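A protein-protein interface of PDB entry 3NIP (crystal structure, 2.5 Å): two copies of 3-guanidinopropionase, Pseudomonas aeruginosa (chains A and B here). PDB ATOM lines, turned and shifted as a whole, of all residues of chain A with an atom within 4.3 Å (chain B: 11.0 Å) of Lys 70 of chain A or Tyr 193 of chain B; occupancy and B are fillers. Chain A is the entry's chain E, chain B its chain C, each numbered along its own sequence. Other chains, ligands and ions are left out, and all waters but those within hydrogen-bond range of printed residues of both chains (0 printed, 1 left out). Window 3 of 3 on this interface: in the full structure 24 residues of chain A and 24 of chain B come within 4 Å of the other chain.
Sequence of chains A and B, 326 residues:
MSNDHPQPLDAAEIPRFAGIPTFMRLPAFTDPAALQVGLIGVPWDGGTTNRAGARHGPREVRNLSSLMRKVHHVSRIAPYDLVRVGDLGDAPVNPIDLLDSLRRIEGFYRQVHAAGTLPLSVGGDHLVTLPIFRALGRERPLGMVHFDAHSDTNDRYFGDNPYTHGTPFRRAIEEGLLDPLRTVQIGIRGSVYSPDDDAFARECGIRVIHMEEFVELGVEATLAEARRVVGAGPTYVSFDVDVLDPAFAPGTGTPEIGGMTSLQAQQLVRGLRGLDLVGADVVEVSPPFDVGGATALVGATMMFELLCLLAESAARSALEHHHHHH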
ATOM      1  N   GLN A   7     -22.270 -43.934   0.747  1.00  0.00           N
ATOM      2  CA  GLN A   7     -22.088 -42.515   0.425  1.00  0.00           C
ATOM      3  C   GLN A   7     -20.755 -42.314  -0.277  1.00  0.00           C
ATOM      4  O   GLN A   7     -19.816 -43.084  -0.054  1.00  0.00           O
ATOM      5  CB  GLN A   7     -22.150 -41.640   1.695  1.00  0.00           C
ATOM      6  CG  GLN A   7     -23.505 -41.606   2.385  1.00  0.00           C
ATOM      7  CD  GLN A   7     -24.549 -40.794   1.636  1.00  0.00           C
ATOM      8  OE1 GLN A   7     -24.221 -39.923   0.829  1.00  0.00           O
ATOM      9  NE2 GLN A   7     -25.821 -41.068   1.912  1.00  0.00           N
ATOM     10  N   PRO A   8     -20.668 -41.284  -1.141  1.00  0.00           N
ATOM     11  CA  PRO A   8     -19.375 -40.887  -1.693  1.00  0.00           C
ATOM     12  C   PRO A   8     -18.431 -40.475  -0.587  1.00  0.00           C
ATOM     13  O   PRO A   8     -18.877 -40.047   0.478  1.00  0.00           O
ATOM     14  CB  PRO A   8     -19.714 -39.649  -2.526  1.00  0.00           C
ATOM     15  CG  PRO A   8     -21.121 -39.797  -2.857  1.00  0.00           C
ATOM     16  CD  PRO A   8     -21.756 -40.444  -1.662  1.00  0.00           C
ATOM     17  N   ASP A  10     -16.384 -38.179   1.603  1.00  0.00           N
ATOM     18  CA  ASP A  10     -16.788 -36.851   2.073  1.00  0.00           C
ATOM     19  C   ASP A  10     -15.830 -35.750   1.598  1.00  0.00           C
ATOM     20  O   ASP A  10     -14.692 -35.654   2.073  1.00  0.00           O
ATOM     21  CB  ASP A  10     -16.903 -36.837   3.603  1.00  0.00           C
ATOM     22  CG  ASP A  10     -17.509 -35.531   4.144  1.00  0.00           C
ATOM     23  OD1 ASP A  10     -18.178 -34.791   3.380  1.00  0.00           O
ATOM     24  OD2 ASP A  10     -17.315 -35.250   5.349  1.00  0.00           O
ATOM     25  N   ALA A  11     -16.310 -34.917   0.678  1.00  0.00           N
ATOM     26  CA  ALA A  11     -15.488 -33.873   0.053  1.00  0.00           C
ATOM     27  C   ALA A  11     -15.056 -32.730   0.993  1.00  0.00           C
ATOM     28  O   ALA A  11     -14.119 -31.990   0.676  1.00  0.00           O
ATOM     29  CB  ALA A  11     -16.180 -33.325  -1.187  1.00  0.00           C
ATOM     30  N   ALA A  12     -15.717 -32.598   2.142  1.00  0.00           N
ATOM     31  CA  ALA A  12     -15.310 -31.629   3.174  1.00  0.00           C
ATOM     32  C   ALA A  12     -14.076 -32.102   3.962  1.00  0.00           C
ATOM     33  O   ALA A  12     -13.459 -31.337   4.718  1.00  0.00           O
ATOM     34  CB  ALA A  12     -16.470 -31.364   4.126  1.00  0.00           C
ATOM     35  N   ARG A  69     -21.017 -34.017  -7.462  1.00  0.00           N
ATOM     36  CA  ARG A  69     -21.440 -33.793  -6.076  1.00  0.00           C
ATOM     37  C   ARG A  69     -22.718 -34.580  -5.776  1.00  0.00           C
ATOM     38  O   ARG A  69     -23.199 -35.323  -6.635  1.00  0.00           O
ATOM     39  CB  ARG A  69     -21.582 -32.291  -5.791  1.00  0.00           C
ATOM     40  CG  ARG A  69     -20.304 -31.530  -6.143  1.00  0.00           C
ATOM     41  CD  ARG A  69     -20.343 -30.049  -5.782  1.00  0.00           C
ATOM     42  NE  ARG A  69     -19.216 -29.364  -6.419  1.00  0.00           N
ATOM     43  CZ  ARG A  69     -19.210 -28.949  -7.686  1.00  0.00           C
ATOM     44  NH1 ARG A  69     -20.263 -29.135  -8.465  1.00  0.00           N
ATOM     45  NH2 ARG A  69     -18.146 -28.343  -8.179  1.00  0.00           N
ATOM     46  N   LYS A  70     -23.261 -34.415  -4.569  1.00  0.00           N
ATOM     47  CA  LYS A  70     -24.290 -35.316  -4.048  1.00  0.00           C
ATOM     48  C   LYS A  70     -25.716 -34.965  -4.440  1.00  0.00           C
ATOM     49  O   LYS A  70     -26.574 -35.837  -4.440  1.00  0.00           O
ATOM     50  CB  LYS A  70     -24.192 -35.427  -2.520  1.00  0.00           C
ATOM     51  CG  LYS A  70     -22.925 -36.124  -1.995  1.00  0.00           C
ATOM     52  CD  LYS A  70     -22.921 -36.225  -0.452  1.00  0.00           C
ATOM     53  CE  LYS A  70     -22.734 -34.861   0.200  1.00  0.00           C
ATOM     54  NZ  LYS A  70     -23.467 -34.707   1.494  1.00  0.00           N
ATOM     55  N   VAL A  71     -25.985 -33.701  -4.767  1.00  0.00           N
ATOM     56  CA  VAL A  71     -27.377 -33.251  -4.988  1.00  0.00           C
ATOM     57  C   VAL A  71     -27.619 -32.541  -6.335  1.00  0.00           C
ATOM     58  O   VAL A  71     -26.895 -31.606  -6.694  1.00  0.00           O
ATOM     59  CB  VAL A  71     -27.881 -32.329  -3.837  1.00  0.00           C
ATOM     60  CG1 VAL A  71     -29.314 -31.891  -4.088  1.00  0.00           C
ATOM     61  CG2 VAL A  71     -27.768 -33.024  -2.473  1.00  0.00           C
ATOM     62  N   ILE A  77     -32.941 -33.958  -6.085  1.00  0.00           N
ATOM     63  CA  ILE A  77     -32.782 -35.377  -5.792  1.00  0.00           C
ATOM     64  C   ILE A  77     -31.414 -35.642  -5.208  1.00  0.00           C
ATOM     65  O   ILE A  77     -30.402 -35.309  -5.810  1.00  0.00           O
ATOM     66  CB  ILE A  77     -32.962 -36.230  -7.072  1.00  0.00           C
ATOM     67  CG1 ILE A  77     -34.427 -36.229  -7.526  1.00  0.00           C
ATOM     68  CG2 ILE A  77     -32.470 -37.665  -6.863  1.00  0.00           C
ATOM     69  CD1 ILE A  77     -34.593 -36.487  -9.046  1.00  0.00           C
ATOM     70  N   ALA A  78     -31.392 -36.230  -4.017  1.00  0.00           N
ATOM     71  CA  ALA A  78     -30.170 -36.724  -3.408  1.00  0.00           C
ATOM     72  C   ALA A  78     -30.193 -38.240  -3.574  1.00  0.00           C
ATOM     73  O   ALA A  78     -30.758 -38.943  -2.731  1.00  0.00           O
ATOM     74  CB  ALA A  78     -30.119 -36.341  -1.960  1.00  0.00           C
ATOM     75  N   PRO A  79     -29.595 -38.749  -4.673  1.00  0.00           N
ATOM     76  CA  PRO A  79     -29.780 -40.161  -5.033  1.00  0.00           C
ATOM     77  C   PRO A  79     -29.230 -41.144  -3.990  1.00  0.00           C
ATOM     78  O   PRO A  79     -29.811 -42.205  -3.773  1.00  0.00           O
ATOM     79  CB  PRO A  79     -29.037 -40.288  -6.379  1.00  0.00           C
ATOM     80  CG  PRO A  79     -28.095 -39.150  -6.422  1.00  0.00           C
ATOM     81  CD  PRO A  79     -28.719 -38.043  -5.633  1.00  0.00           C
ATOM     82  N   TYR A  80     -28.133 -40.777  -3.340  1.00  0.00           N
ATOM     83  CA  TYR A  80     -27.515 -41.638  -2.335  1.00  0.00           C
ATOM     84  C   TYR A  80     -28.329 -41.716  -1.046  1.00  0.00           C
ATOM     85  O   TYR A  80     -28.243 -42.714  -0.335  1.00  0.00           O
ATOM     86  CB  TYR A  80     -26.055 -41.230  -2.082  1.00  0.00           C
ATOM     87  CG  TYR A  80     -25.340 -40.923  -3.375  1.00  0.00           C
ATOM     88  CD1 TYR A  80     -25.374 -41.829  -4.437  1.00  0.00           C
ATOM     89  CD2 TYR A  80     -24.665 -39.711  -3.565  1.00  0.00           C
ATOM     90  CE1 TYR A  80     -24.740 -41.539  -5.650  1.00  0.00           C
ATOM     91  CE2 TYR A  80     -24.027 -39.413  -4.788  1.00  0.00           C
ATOM     92  CZ  TYR A  80     -24.075 -40.332  -5.815  1.00  0.00           C
ATOM     93  OH  TYR A  80     -23.454 -40.084  -7.015  1.00  0.00           O
ATOM     94  N   PHE A 304     -24.566 -39.036 -13.860  1.00  0.00           N
ATOM     95  CA  PHE A 304     -25.229 -38.477 -12.696  1.00  0.00           C
ATOM     96  C   PHE A 304     -26.664 -38.079 -13.000  1.00  0.00           C
ATOM     97  O   PHE A 304     -27.552 -38.354 -12.205  1.00  0.00           O
ATOM     98  CB  PHE A 304     -24.470 -37.280 -12.115  1.00  0.00           C
ATOM     99  CG  PHE A 304     -25.045 -36.790 -10.809  1.00  0.00           C
ATOM    100  CD1 PHE A 304     -24.712 -37.421  -9.602  1.00  0.00           C
ATOM    101  CD2 PHE A 304     -25.935 -35.724 -10.786  1.00  0.00           C
ATOM    102  CE1 PHE A 304     -25.255 -36.988  -8.392  1.00  0.00           C
ATOM    103  CE2 PHE A 304     -26.489 -35.288  -9.579  1.00  0.00           C
ATOM    104  CZ  PHE A 304     -26.154 -35.922  -8.381  1.00  0.00           C
ATOM    105  N   THR B  49      -9.004 -25.734  -4.456  1.00  0.00           N
ATOM    106  CA  THR B  49      -9.119 -26.938  -3.631  1.00  0.00           C
ATOM    107  C   THR B  49      -8.923 -28.237  -4.403  1.00  0.00           C
ATOM    108  O   THR B  49      -8.747 -29.293  -3.804  1.00  0.00           O
ATOM    109  CB  THR B  49     -10.478 -26.994  -2.875  1.00  0.00           C
ATOM    110  OG1 THR B  49     -11.556 -26.855  -3.808  1.00  0.00           O
ATOM    111  CG2 THR B  49     -10.569 -25.875  -1.838  1.00  0.00           C
ATOM    112  N   ALA B 149     -20.323 -20.349 -12.986  1.00  0.00           N
ATOM    113  CA  ALA B 149     -21.036 -21.600 -12.756  1.00  0.00           C
ATOM    114  C   ALA B 149     -21.359 -21.791 -11.266  1.00  0.00           C
ATOM    115  O   ALA B 149     -22.272 -22.534 -10.930  1.00  0.00           O
ATOM    116  CB  ALA B 149     -20.247 -22.790 -13.306  1.00  0.00           C
ATOM    117  N   HIS B 150     -20.632 -21.096 -10.391  1.00  0.00           N
ATOM    118  CA  HIS B 150     -20.807 -21.227  -8.939  1.00  0.00           C
ATOM    119  C   HIS B 150     -21.007 -19.889  -8.253  1.00  0.00           C
ATOM    120  O   HIS B 150     -20.416 -18.892  -8.658  1.00  0.00           O
ATOM    121  CB  HIS B 150     -19.586 -21.909  -8.314  1.00  0.00           C
ATOM    122  CG  HIS B 150     -19.074 -23.054  -9.119  1.00  0.00           C
ATOM    123  ND1 HIS B 150     -17.969 -22.948  -9.941  1.00  0.00           N
ATOM    124  CD2 HIS B 150     -19.545 -24.316  -9.272  1.00  0.00           C
ATOM    125  CE1 HIS B 150     -17.774 -24.103 -10.553  1.00  0.00           C
ATOM    126  NE2 HIS B 150     -18.710 -24.953 -10.158  1.00  0.00           N
ATOM    127  N   SER B 151     -21.808 -19.879  -7.192  1.00  0.00           N
ATOM    128  CA  SER B 151     -22.025 -18.661  -6.392  1.00  0.00           C
ATOM    129  C   SER B 151     -20.794 -18.115  -5.687  1.00  0.00           C
ATOM    130  O   SER B 151     -20.734 -16.922  -5.431  1.00  0.00           O
ATOM    131  CB  SER B 151     -23.124 -18.869  -5.340  1.00  0.00           C
ATOM    132  OG  SER B 151     -24.386 -18.928  -5.958  1.00  0.00           O
ATOM    133  N   ASN B 154     -19.819 -19.847  -0.410  1.00  0.00           N
ATOM    134  CA  ASN B 154     -19.673 -20.866   0.635  1.00  0.00           C
ATOM    135  C   ASN B 154     -18.904 -20.327   1.824  1.00  0.00           C
ATOM    136  O   ASN B 154     -18.286 -19.260   1.755  1.00  0.00           O
ATOM    137  CB  ASN B 154     -19.005 -22.133   0.101  1.00  0.00           C
ATOM    138  CG  ASN B 154     -19.798 -22.775  -1.021  1.00  0.00           C
ATOM    139  OD1 ASN B 154     -20.978 -23.101  -0.859  1.00  0.00           O
ATOM    140  ND2 ASN B 154     -19.156 -22.942  -2.179  1.00  0.00           N
ATOM    141  N   ASP B 155     -18.928 -21.083   2.915  1.00  0.00           N
ATOM    142  CA  ASP B 155     -18.485 -20.568   4.196  1.00  0.00           C
ATOM    143  C   ASP B 155     -17.069 -21.017   4.563  1.00  0.00           C
ATOM    144  O   ASP B 155     -16.185 -20.185   4.696  1.00  0.00           O
ATOM    145  CB  ASP B 155     -19.511 -20.939   5.282  1.00  0.00           C
ATOM    146  CG  ASP B 155     -19.182 -20.332   6.643  1.00  0.00           C
ATOM    147  OD1 ASP B 155     -18.658 -19.188   6.707  1.00  0.00           O
ATOM    148  OD2 ASP B 155     -19.459 -21.012   7.658  1.00  0.00           O
ATOM    149  N   ARG B 156     -16.869 -22.329   4.709  1.00  0.00           N
ATOM    150  CA  ARG B 156     -15.635 -22.907   5.263  1.00  0.00           C
ATOM    151  C   ARG B 156     -15.203 -24.126   4.452  1.00  0.00           C
ATOM    152  O   ARG B 156     -16.043 -24.880   3.960  1.00  0.00           O
ATOM    153  CB  ARG B 156     -15.859 -23.364   6.713  1.00  0.00           C
ATOM    154  CG  ARG B 156     -16.012 -22.266   7.765  1.00  0.00           C
ATOM    155  CD  ARG B 156     -14.794 -21.351   7.775  1.00  0.00           C
ATOM    156  NE  ARG B 156     -14.600 -20.645   9.041  1.00  0.00           N
ATOM    157  CZ  ARG B 156     -14.866 -19.352   9.244  1.00  0.00           C
ATOM    158  NH1 ARG B 156     -15.359 -18.595   8.264  1.00  0.00           N
ATOM    159  NH2 ARG B 156     -14.630 -18.806  10.435  1.00  0.00           N
ATOM    160  N   TYR B 157     -13.896 -24.335   4.338  1.00  0.00           N
ATOM    161  CA  TYR B 157     -13.377 -25.546   3.705  1.00  0.00           C
ATOM    162  C   TYR B 157     -12.378 -26.299   4.576  1.00  0.00           C
ATOM    163  O   TYR B 157     -11.538 -25.688   5.260  1.00  0.00           O
ATOM    164  CB  TYR B 157     -12.766 -25.251   2.329  1.00  0.00           C
ATOM    165  CG  TYR B 157     -13.790 -24.972   1.246  1.00  0.00           C
ATOM    166  CD1 TYR B 157     -14.275 -25.996   0.426  1.00  0.00           C
ATOM    167  CD2 TYR B 157     -14.278 -23.679   1.036  1.00  0.00           C
ATOM    168  CE1 TYR B 157     -15.223 -25.728  -0.582  1.00  0.00           C
ATOM    169  CE2 TYR B 157     -15.215 -23.407   0.037  1.00  0.00           C
ATOM    170  CZ  TYR B 157     -15.683 -24.425  -0.763  1.00  0.00           C
ATOM    171  OH  TYR B 157     -16.614 -24.130  -1.733  1.00  0.00           O
ATOM    172  N   PHE B 158     -12.494 -27.629   4.539  1.00  0.00           N
ATOM    173  CA  PHE B 158     -11.582 -28.560   5.218  1.00  0.00           C
ATOM    174  C   PHE B 158     -11.291 -28.145   6.659  1.00  0.00           C
ATOM    175  O   PHE B 158     -10.143 -28.045   7.079  1.00  0.00           O
ATOM    176  CB  PHE B 158     -10.295 -28.761   4.398  1.00  0.00           C
ATOM    177  CG  PHE B 158     -10.540 -29.199   2.969  1.00  0.00           C
ATOM    178  CD1 PHE B 158     -10.717 -30.554   2.661  1.00  0.00           C
ATOM    179  CD2 PHE B 158     -10.594 -28.251   1.929  1.00  0.00           C
ATOM    180  CE1 PHE B 158     -10.949 -30.962   1.331  1.00  0.00           C
ATOM    181  CE2 PHE B 158     -10.827 -28.642   0.600  1.00  0.00           C
ATOM    182  CZ  PHE B 158     -11.000 -29.996   0.292  1.00  0.00           C
ATOM    183  N   GLY B 159     -12.354 -27.924   7.419  1.00  0.00           N
ATOM    184  CA  GLY B 159     -12.234 -27.340   8.749  1.00  0.00           C
ATOM    185  C   GLY B 159     -12.667 -25.894   8.639  1.00  0.00           C
ATOM    186  O   GLY B 159     -13.619 -25.588   7.912  1.00  0.00           O
ATOM    187  N   GLY B 166     -14.082 -20.585  -3.762  1.00  0.00           N
ATOM    188  CA  GLY B 166     -15.523 -20.691  -3.520  1.00  0.00           C
ATOM    189  C   GLY B 166     -16.108 -19.896  -2.350  1.00  0.00           C
ATOM    190  O   GLY B 166     -17.319 -20.002  -2.075  1.00  0.00           O
ATOM    191  N   ILE B 188     -25.309 -20.095 -12.891  1.00  0.00           N
ATOM    192  CA  ILE B 188     -25.072 -21.074 -11.819  1.00  0.00           C
ATOM    193  C   ILE B 188     -25.647 -22.441 -12.177  1.00  0.00           C
ATOM    194  O   ILE B 188     -26.800 -22.541 -12.589  1.00  0.00           O
ATOM    195  CB  ILE B 188     -25.671 -20.570 -10.464  1.00  0.00           C
ATOM    196  CG1 ILE B 188     -25.238 -19.122 -10.164  1.00  0.00           C
ATOM    197  CG2 ILE B 188     -25.349 -21.534  -9.293  1.00  0.00           C
ATOM    198  CD1 ILE B 188     -23.735 -18.880 -10.200  1.00  0.00           C
ATOM    199  N   ARG B 189     -24.842 -23.486 -12.036  1.00  0.00           N
ATOM    200  CA  ARG B 189     -25.247 -24.822 -12.463  1.00  0.00           C
ATOM    201  C   ARG B 189     -24.330 -25.883 -11.874  1.00  0.00           C
ATOM    202  O   ARG B 189     -23.201 -25.588 -11.469  1.00  0.00           O
ATOM    203  CB  ARG B 189     -25.228 -24.926 -13.993  1.00  0.00           C
ATOM    204  CG  ARG B 189     -23.827 -24.787 -14.613  1.00  0.00           C
ATOM    205  CD  ARG B 189     -23.861 -24.793 -16.135  1.00  0.00           C
ATOM    206  NE  ARG B 189     -22.528 -24.830 -16.745  1.00  0.00           N
ATOM    207  CZ  ARG B 189     -21.770 -23.760 -16.959  1.00  0.00           C
ATOM    208  NH1 ARG B 189     -22.192 -22.559 -16.619  1.00  0.00           N
ATOM    209  NH2 ARG B 189     -20.592 -23.888 -17.524  1.00  0.00           N
ATOM    210  N   GLY B 190     -24.825 -27.121 -11.837  1.00  0.00           N
ATOM    211  CA  GLY B 190     -24.032 -28.271 -11.433  1.00  0.00           C
ATOM    212  C   GLY B 190     -24.503 -28.861 -10.130  1.00  0.00           C
ATOM    213  O   GLY B 190     -25.139 -28.173  -9.330  1.00  0.00           O
ATOM    214  N   SER B 191     -24.183 -30.136  -9.911  1.00  0.00           N
ATOM    215  CA  SER B 191     -24.537 -30.804  -8.675  1.00  0.00           C
ATOM    216  C   SER B 191     -23.990 -30.033  -7.470  1.00  0.00           C
ATOM    217  O   SER B 191     -22.913 -29.442  -7.528  1.00  0.00           O
ATOM    218  CB  SER B 191     -24.017 -32.240  -8.677  1.00  0.00           C
ATOM    219  OG  SER B 191     -22.607 -32.280  -8.787  1.00  0.00           O
ATOM    220  N   VAL B 192     -24.751 -30.021  -6.385  1.00  0.00           N
ATOM    221  CA  VAL B 192     -24.319 -29.337  -5.178  1.00  0.00           C
ATOM    222  C   VAL B 192     -24.089 -30.313  -4.043  1.00  0.00           C
ATOM    223  O   VAL B 192     -24.571 -31.444  -4.069  1.00  0.00           O
ATOM    224  CB  VAL B 192     -25.300 -28.216  -4.746  1.00  0.00           C
ATOM    225  CG1 VAL B 192     -25.201 -27.016  -5.708  1.00  0.00           C
ATOM    226  CG2 VAL B 192     -26.712 -28.743  -4.663  1.00  0.00           C
ATOM    227  N   TYR B 193     -23.332 -29.855  -3.056  1.00  0.00           N
ATOM    228  CA  TYR B 193     -22.935 -30.652  -1.904  1.00  0.00           C
ATOM    229  C   TYR B 193     -24.127 -30.946  -0.970  1.00  0.00           C
ATOM    230  O   TYR B 193     -24.197 -32.026  -0.376  1.00  0.00           O
ATOM    231  CB  TYR B 193     -21.800 -29.915  -1.183  1.00  0.00           C
ATOM    232  CG  TYR B 193     -21.216 -30.590   0.038  1.00  0.00           C
ATOM    233  CD1 TYR B 193     -20.055 -31.366  -0.059  1.00  0.00           C
ATOM    234  CD2 TYR B 193     -21.797 -30.420   1.308  1.00  0.00           C
ATOM    235  CE1 TYR B 193     -19.500 -31.981   1.075  1.00  0.00           C
ATOM    236  CE2 TYR B 193     -21.255 -31.029   2.440  1.00  0.00           C
ATOM    237  CZ  TYR B 193     -20.106 -31.808   2.315  1.00  0.00           C
ATOM    238  OH  TYR B 193     -19.564 -32.408   3.430  1.00  0.00           O
ATOM    239  N   SER B 194     -25.076 -30.012  -0.888  1.00  0.00           N
ATOM    240  CA  SER B 194     -26.116 -30.036   0.150  1.00  0.00           C
ATOM    241  C   SER B 194     -27.541 -29.805  -0.365  1.00  0.00           C
ATOM    242  O   SER B 194     -27.742 -28.971  -1.247  1.00  0.00           O
ATOM    243  CB  SER B 194     -25.775 -29.011   1.251  1.00  0.00           C
ATOM    244  OG  SER B 194     -25.783 -27.680   0.752  1.00  0.00           O
ATOM    245  N   PRO B 195     -28.534 -30.529   0.217  1.00  0.00           N
ATOM    246  CA  PRO B 195     -29.968 -30.521  -0.162  1.00  0.00           C
ATOM    247  C   PRO B 195     -30.605 -29.141  -0.368  1.00  0.00           C
ATOM    248  O   PRO B 195     -31.612 -29.026  -1.088  1.00  0.00           O
ATOM    249  CB  PRO B 195     -30.635 -31.250   1.010  1.00  0.00           C
ATOM    250  CG  PRO B 195     -29.610 -32.261   1.419  1.00  0.00           C
ATOM    251  CD  PRO B 195     -28.271 -31.556   1.254  1.00  0.00           C
ATOM    252  N   ASP B 196     -30.041 -28.122   0.282  1.00  0.00           N
ATOM    253  CA  ASP B 196     -30.367 -26.728  -0.023  1.00  0.00           C
ATOM    254  C   ASP B 196     -29.067 -25.932  -0.052  1.00  0.00           C
ATOM    255  O   ASP B 196     -28.294 -25.925   0.931  1.00  0.00           O
ATOM    256  CB  ASP B 196     -31.380 -26.118   0.967  1.00  0.00           C
ATOM    257  CG  ASP B 196     -32.195 -24.963   0.350  1.00  0.00           C
ATOM    258  OD1 ASP B 196     -31.903 -24.539  -0.797  1.00  0.00           O
ATOM    259  OD2 ASP B 196     -33.143 -24.481   1.017  1.00  0.00           O
ATOM    260  N   ASP B 197     -28.840 -25.276  -1.195  1.00  0.00           N
ATOM    261  CA  ASP B 197     -27.569 -24.633  -1.508  1.00  0.00           C
ATOM    262  C   ASP B 197     -27.629 -23.103  -1.440  1.00  0.00           C
ATOM    263  O   ASP B 197     -26.795 -22.465  -0.791  1.00  0.00           O
ATOM    264  CB  ASP B 197     -27.106 -25.060  -2.895  1.00  0.00           C
ATOM    265  CG  ASP B 197     -25.660 -24.720  -3.135  1.00  0.00           C
ATOM    266  OD1 ASP B 197     -24.793 -25.509  -2.696  1.00  0.00           O
ATOM    267  OD2 ASP B 197     -25.387 -23.664  -3.750  1.00  0.00           O
ATOM    268  N   ASP B 198     -28.626 -22.530  -2.110  1.00  0.00           N
ATOM    269  CA  ASP B 198     -28.797 -21.086  -2.179  1.00  0.00           C
ATOM    270  C   ASP B 198     -29.333 -20.534  -0.845  1.00  0.00           C
ATOM    271  O   ASP B 198     -30.103 -19.563  -0.817  1.00  0.00           O
ATOM    272  CB  ASP B 198     -29.721 -20.720  -3.354  1.00  0.00           C
ATOM    273  CG  ASP B 198     -29.251 -21.322  -4.691  1.00  0.00           C
ATOM    274  OD1 ASP B 198     -29.798 -22.380  -5.098  1.00  0.00           O
ATOM    275  OD2 ASP B 198     -28.333 -20.748  -5.323  1.00  0.00           O
ATOM    276  N   ALA B 199     -28.908 -21.161   0.254  1.00  0.00           N
ATOM    277  CA  ALA B 199     -29.343 -20.786   1.592  1.00  0.00           C
ATOM    278  C   ALA B 199     -28.857 -19.381   1.901  1.00  0.00           C
ATOM    279  O   ALA B 199     -29.664 -18.471   2.101  1.00  0.00           O
ATOM    280  CB  ALA B 199     -28.823 -21.789   2.631  1.00  0.00           C
ATOM    281  N   THR B 254     -12.749 -25.891 -12.356  1.00  0.00           N
ATOM    282  CA  THR B 254     -14.003 -26.509 -11.934  1.00  0.00           C
ATOM    283  C   THR B 254     -15.097 -26.374 -12.994  1.00  0.00           C
ATOM    284  O   THR B 254     -16.056 -25.608 -12.819  1.00  0.00           O
ATOM    285  CB  THR B 254     -14.502 -25.943 -10.577  1.00  0.00           C
ATOM    286  OG1 THR B 254     -13.389 -25.772  -9.695  1.00  0.00           O
ATOM    287  CG2 THR B 254     -15.498 -26.888  -9.922  1.00  0.00           C
ATOM    288  N   GLU B 256     -18.363 -27.203 -15.367  1.00  0.00           N
ATOM    289  CA  GLU B 256     -19.680 -27.781 -15.247  1.00  0.00           C
ATOM    290  C   GLU B 256     -20.223 -27.714 -16.650  1.00  0.00           C
ATOM    291  O   GLU B 256     -20.290 -26.620 -17.232  1.00  0.00           O
ATOM    292  CB  GLU B 256     -20.589 -26.967 -14.305  1.00  0.00           C
ATOM    293  CG  GLU B 256     -19.993 -26.623 -12.936  1.00  0.00           C
ATOM    294  CD  GLU B 256     -19.851 -27.817 -11.994  1.00  0.00           C
ATOM    295  OE1 GLU B 256     -20.447 -28.889 -12.239  1.00  0.00           O
ATOM    296  OE2 GLU B 256     -19.141 -27.673 -10.982  1.00  0.00           O
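O of Val 71 of chain A sits at hydrogen-bond distance from N of Val 192 of chain B, at 2.7 Å.
The backbone carbonyl oxygen (O) of Val 192 of chain B lies within hydrogen-bond range of the backbone NH (N) of Lys 70 of chain A.
OE2 of Glu 256 of chain B lies within salt-bridge range of NH2 of Arg 69 of chain A, 3.0 Å away.
O of Tyr 193 of chain B sits close to NZ of Lys 70 of chain A.
N of Arg 69 of chain A is in hydrogen-bond range of OG of Ser 191 of chain B (2.7 Å).
The side-chain hydroxyl (OH) of Tyr 193 of chain B is in hydrogen-bond range of the side-chain carboxylate (OD1) of Asp 10 of chain A (2.8 Å).
NH2 of Arg 189 of chain B lies within hydrogen-bond range of O of Glu 256 of chain B.
The side-chain hydroxyl (OG) of Ser 194 of chain B lies within hydrogen-bond range of the backbone carbonyl oxygen (O) of Asp 196 of chain B (3.1 Å).
The side-chain carboxylate of Glu 256 of chain B sits at hydrogen-bond distance from a ring nitrogen (NE2) of His 150 of chain B (2.9 Å).
Ala 11 of chain A touches Phe 158 of chain B (O to CE1, 3.4 Å).
Phe 158 of chain B touches Ala 12 of chain A.
Ala 12 of chain A touches Tyr 193 of chain B.
Arg 69 of chain A touches His 150 of chain B (NH2 to NE2, 3.97 Å).
CB of Arg 69 of chain A touches O of Val 192 of chain B, at 3.6 Å.
CG2 of Thr 254 of chain B touches NH2 of Arg 69 of chain A, 3.5 Å away.
Val 71 of chain A touches Ser 191 of chain B (O to CA, 3.2 Å).
Val 71 of chain A touches Ser 194 of chain B.
CG2 of Val 71 of chain A touches N of Pro 195 of chain B, at 3.7 Å.
Lys 70 of chain A touches just these residues of chain B: Val 192 and Tyr 193.
No residue of chain B comes within 4 Å of Pro 8 of chain A.
Of chain B, only Tyr 193 comes within 4 Å of Asp 10 of chain A.
Of chain B, only Phe 158 (3.4 Å) comes within 4 Å of Ala 11 of chain A.
Val 71 of chain A touches just these residues of chain B: Ser 191, Val 192, Ser 194 and Pro 195.
No residue of chain B comes within 4 Å of Ala 78 of chain A.
Printed residues of chain A within 4 Å of Phe 158 of chain B: Ala 11 (3.4 Å) and Ala 12 (3.4 Å).
Of the printed residues of chain A, Ser 194 of chain B touches Val 71 (3.9 Å).
Of the printed residues of chain A, Val 192 of chain B touches Arg 69, Lys 70 and Val 71.
Printed residues of chain A within 4 Å of His 150 of chain B: Arg 69 (3.97 Å).
The nearest residue of chain A that does not touch Tyr 193 of chain B is Arg 69 of chain A (4.1 Å).
The nearest printed residue of chain A that does not touch Phe 158 of chain B is Asp 10 of chain A (6.0 Å).
Of the 25 printed residues of chain B, 9 touch a printed residue of chain A.
Printed residues of chain B that touch a printed residue of chain A: His 150, Phe 158, Ser 191, Val 192, Tyr 193, Ser 194, Pro 195, Thr 254 and Glu 256.
Hydrophobic or aromatic side chains of chain B that line the printed part of chain A: His 150, Phe 158, Val 192 and Tyr 193.
Of the 13 printed residues of chain A, 6 touch a printed residue of chain B.
Among the printed residues, 15 pairs touch across the chains.
Among the printed residues, Asp or Glu carboxylates within 4 Å of a Lys or Arg side-chain nitrogen of the other chain: Arg 69 of chain A with Glu 256 of chain B.
No position is printed for both chains.
Of the 15 pairs that touch across the chains among the printed residues, none has its exchanged pair printed and touching as well.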
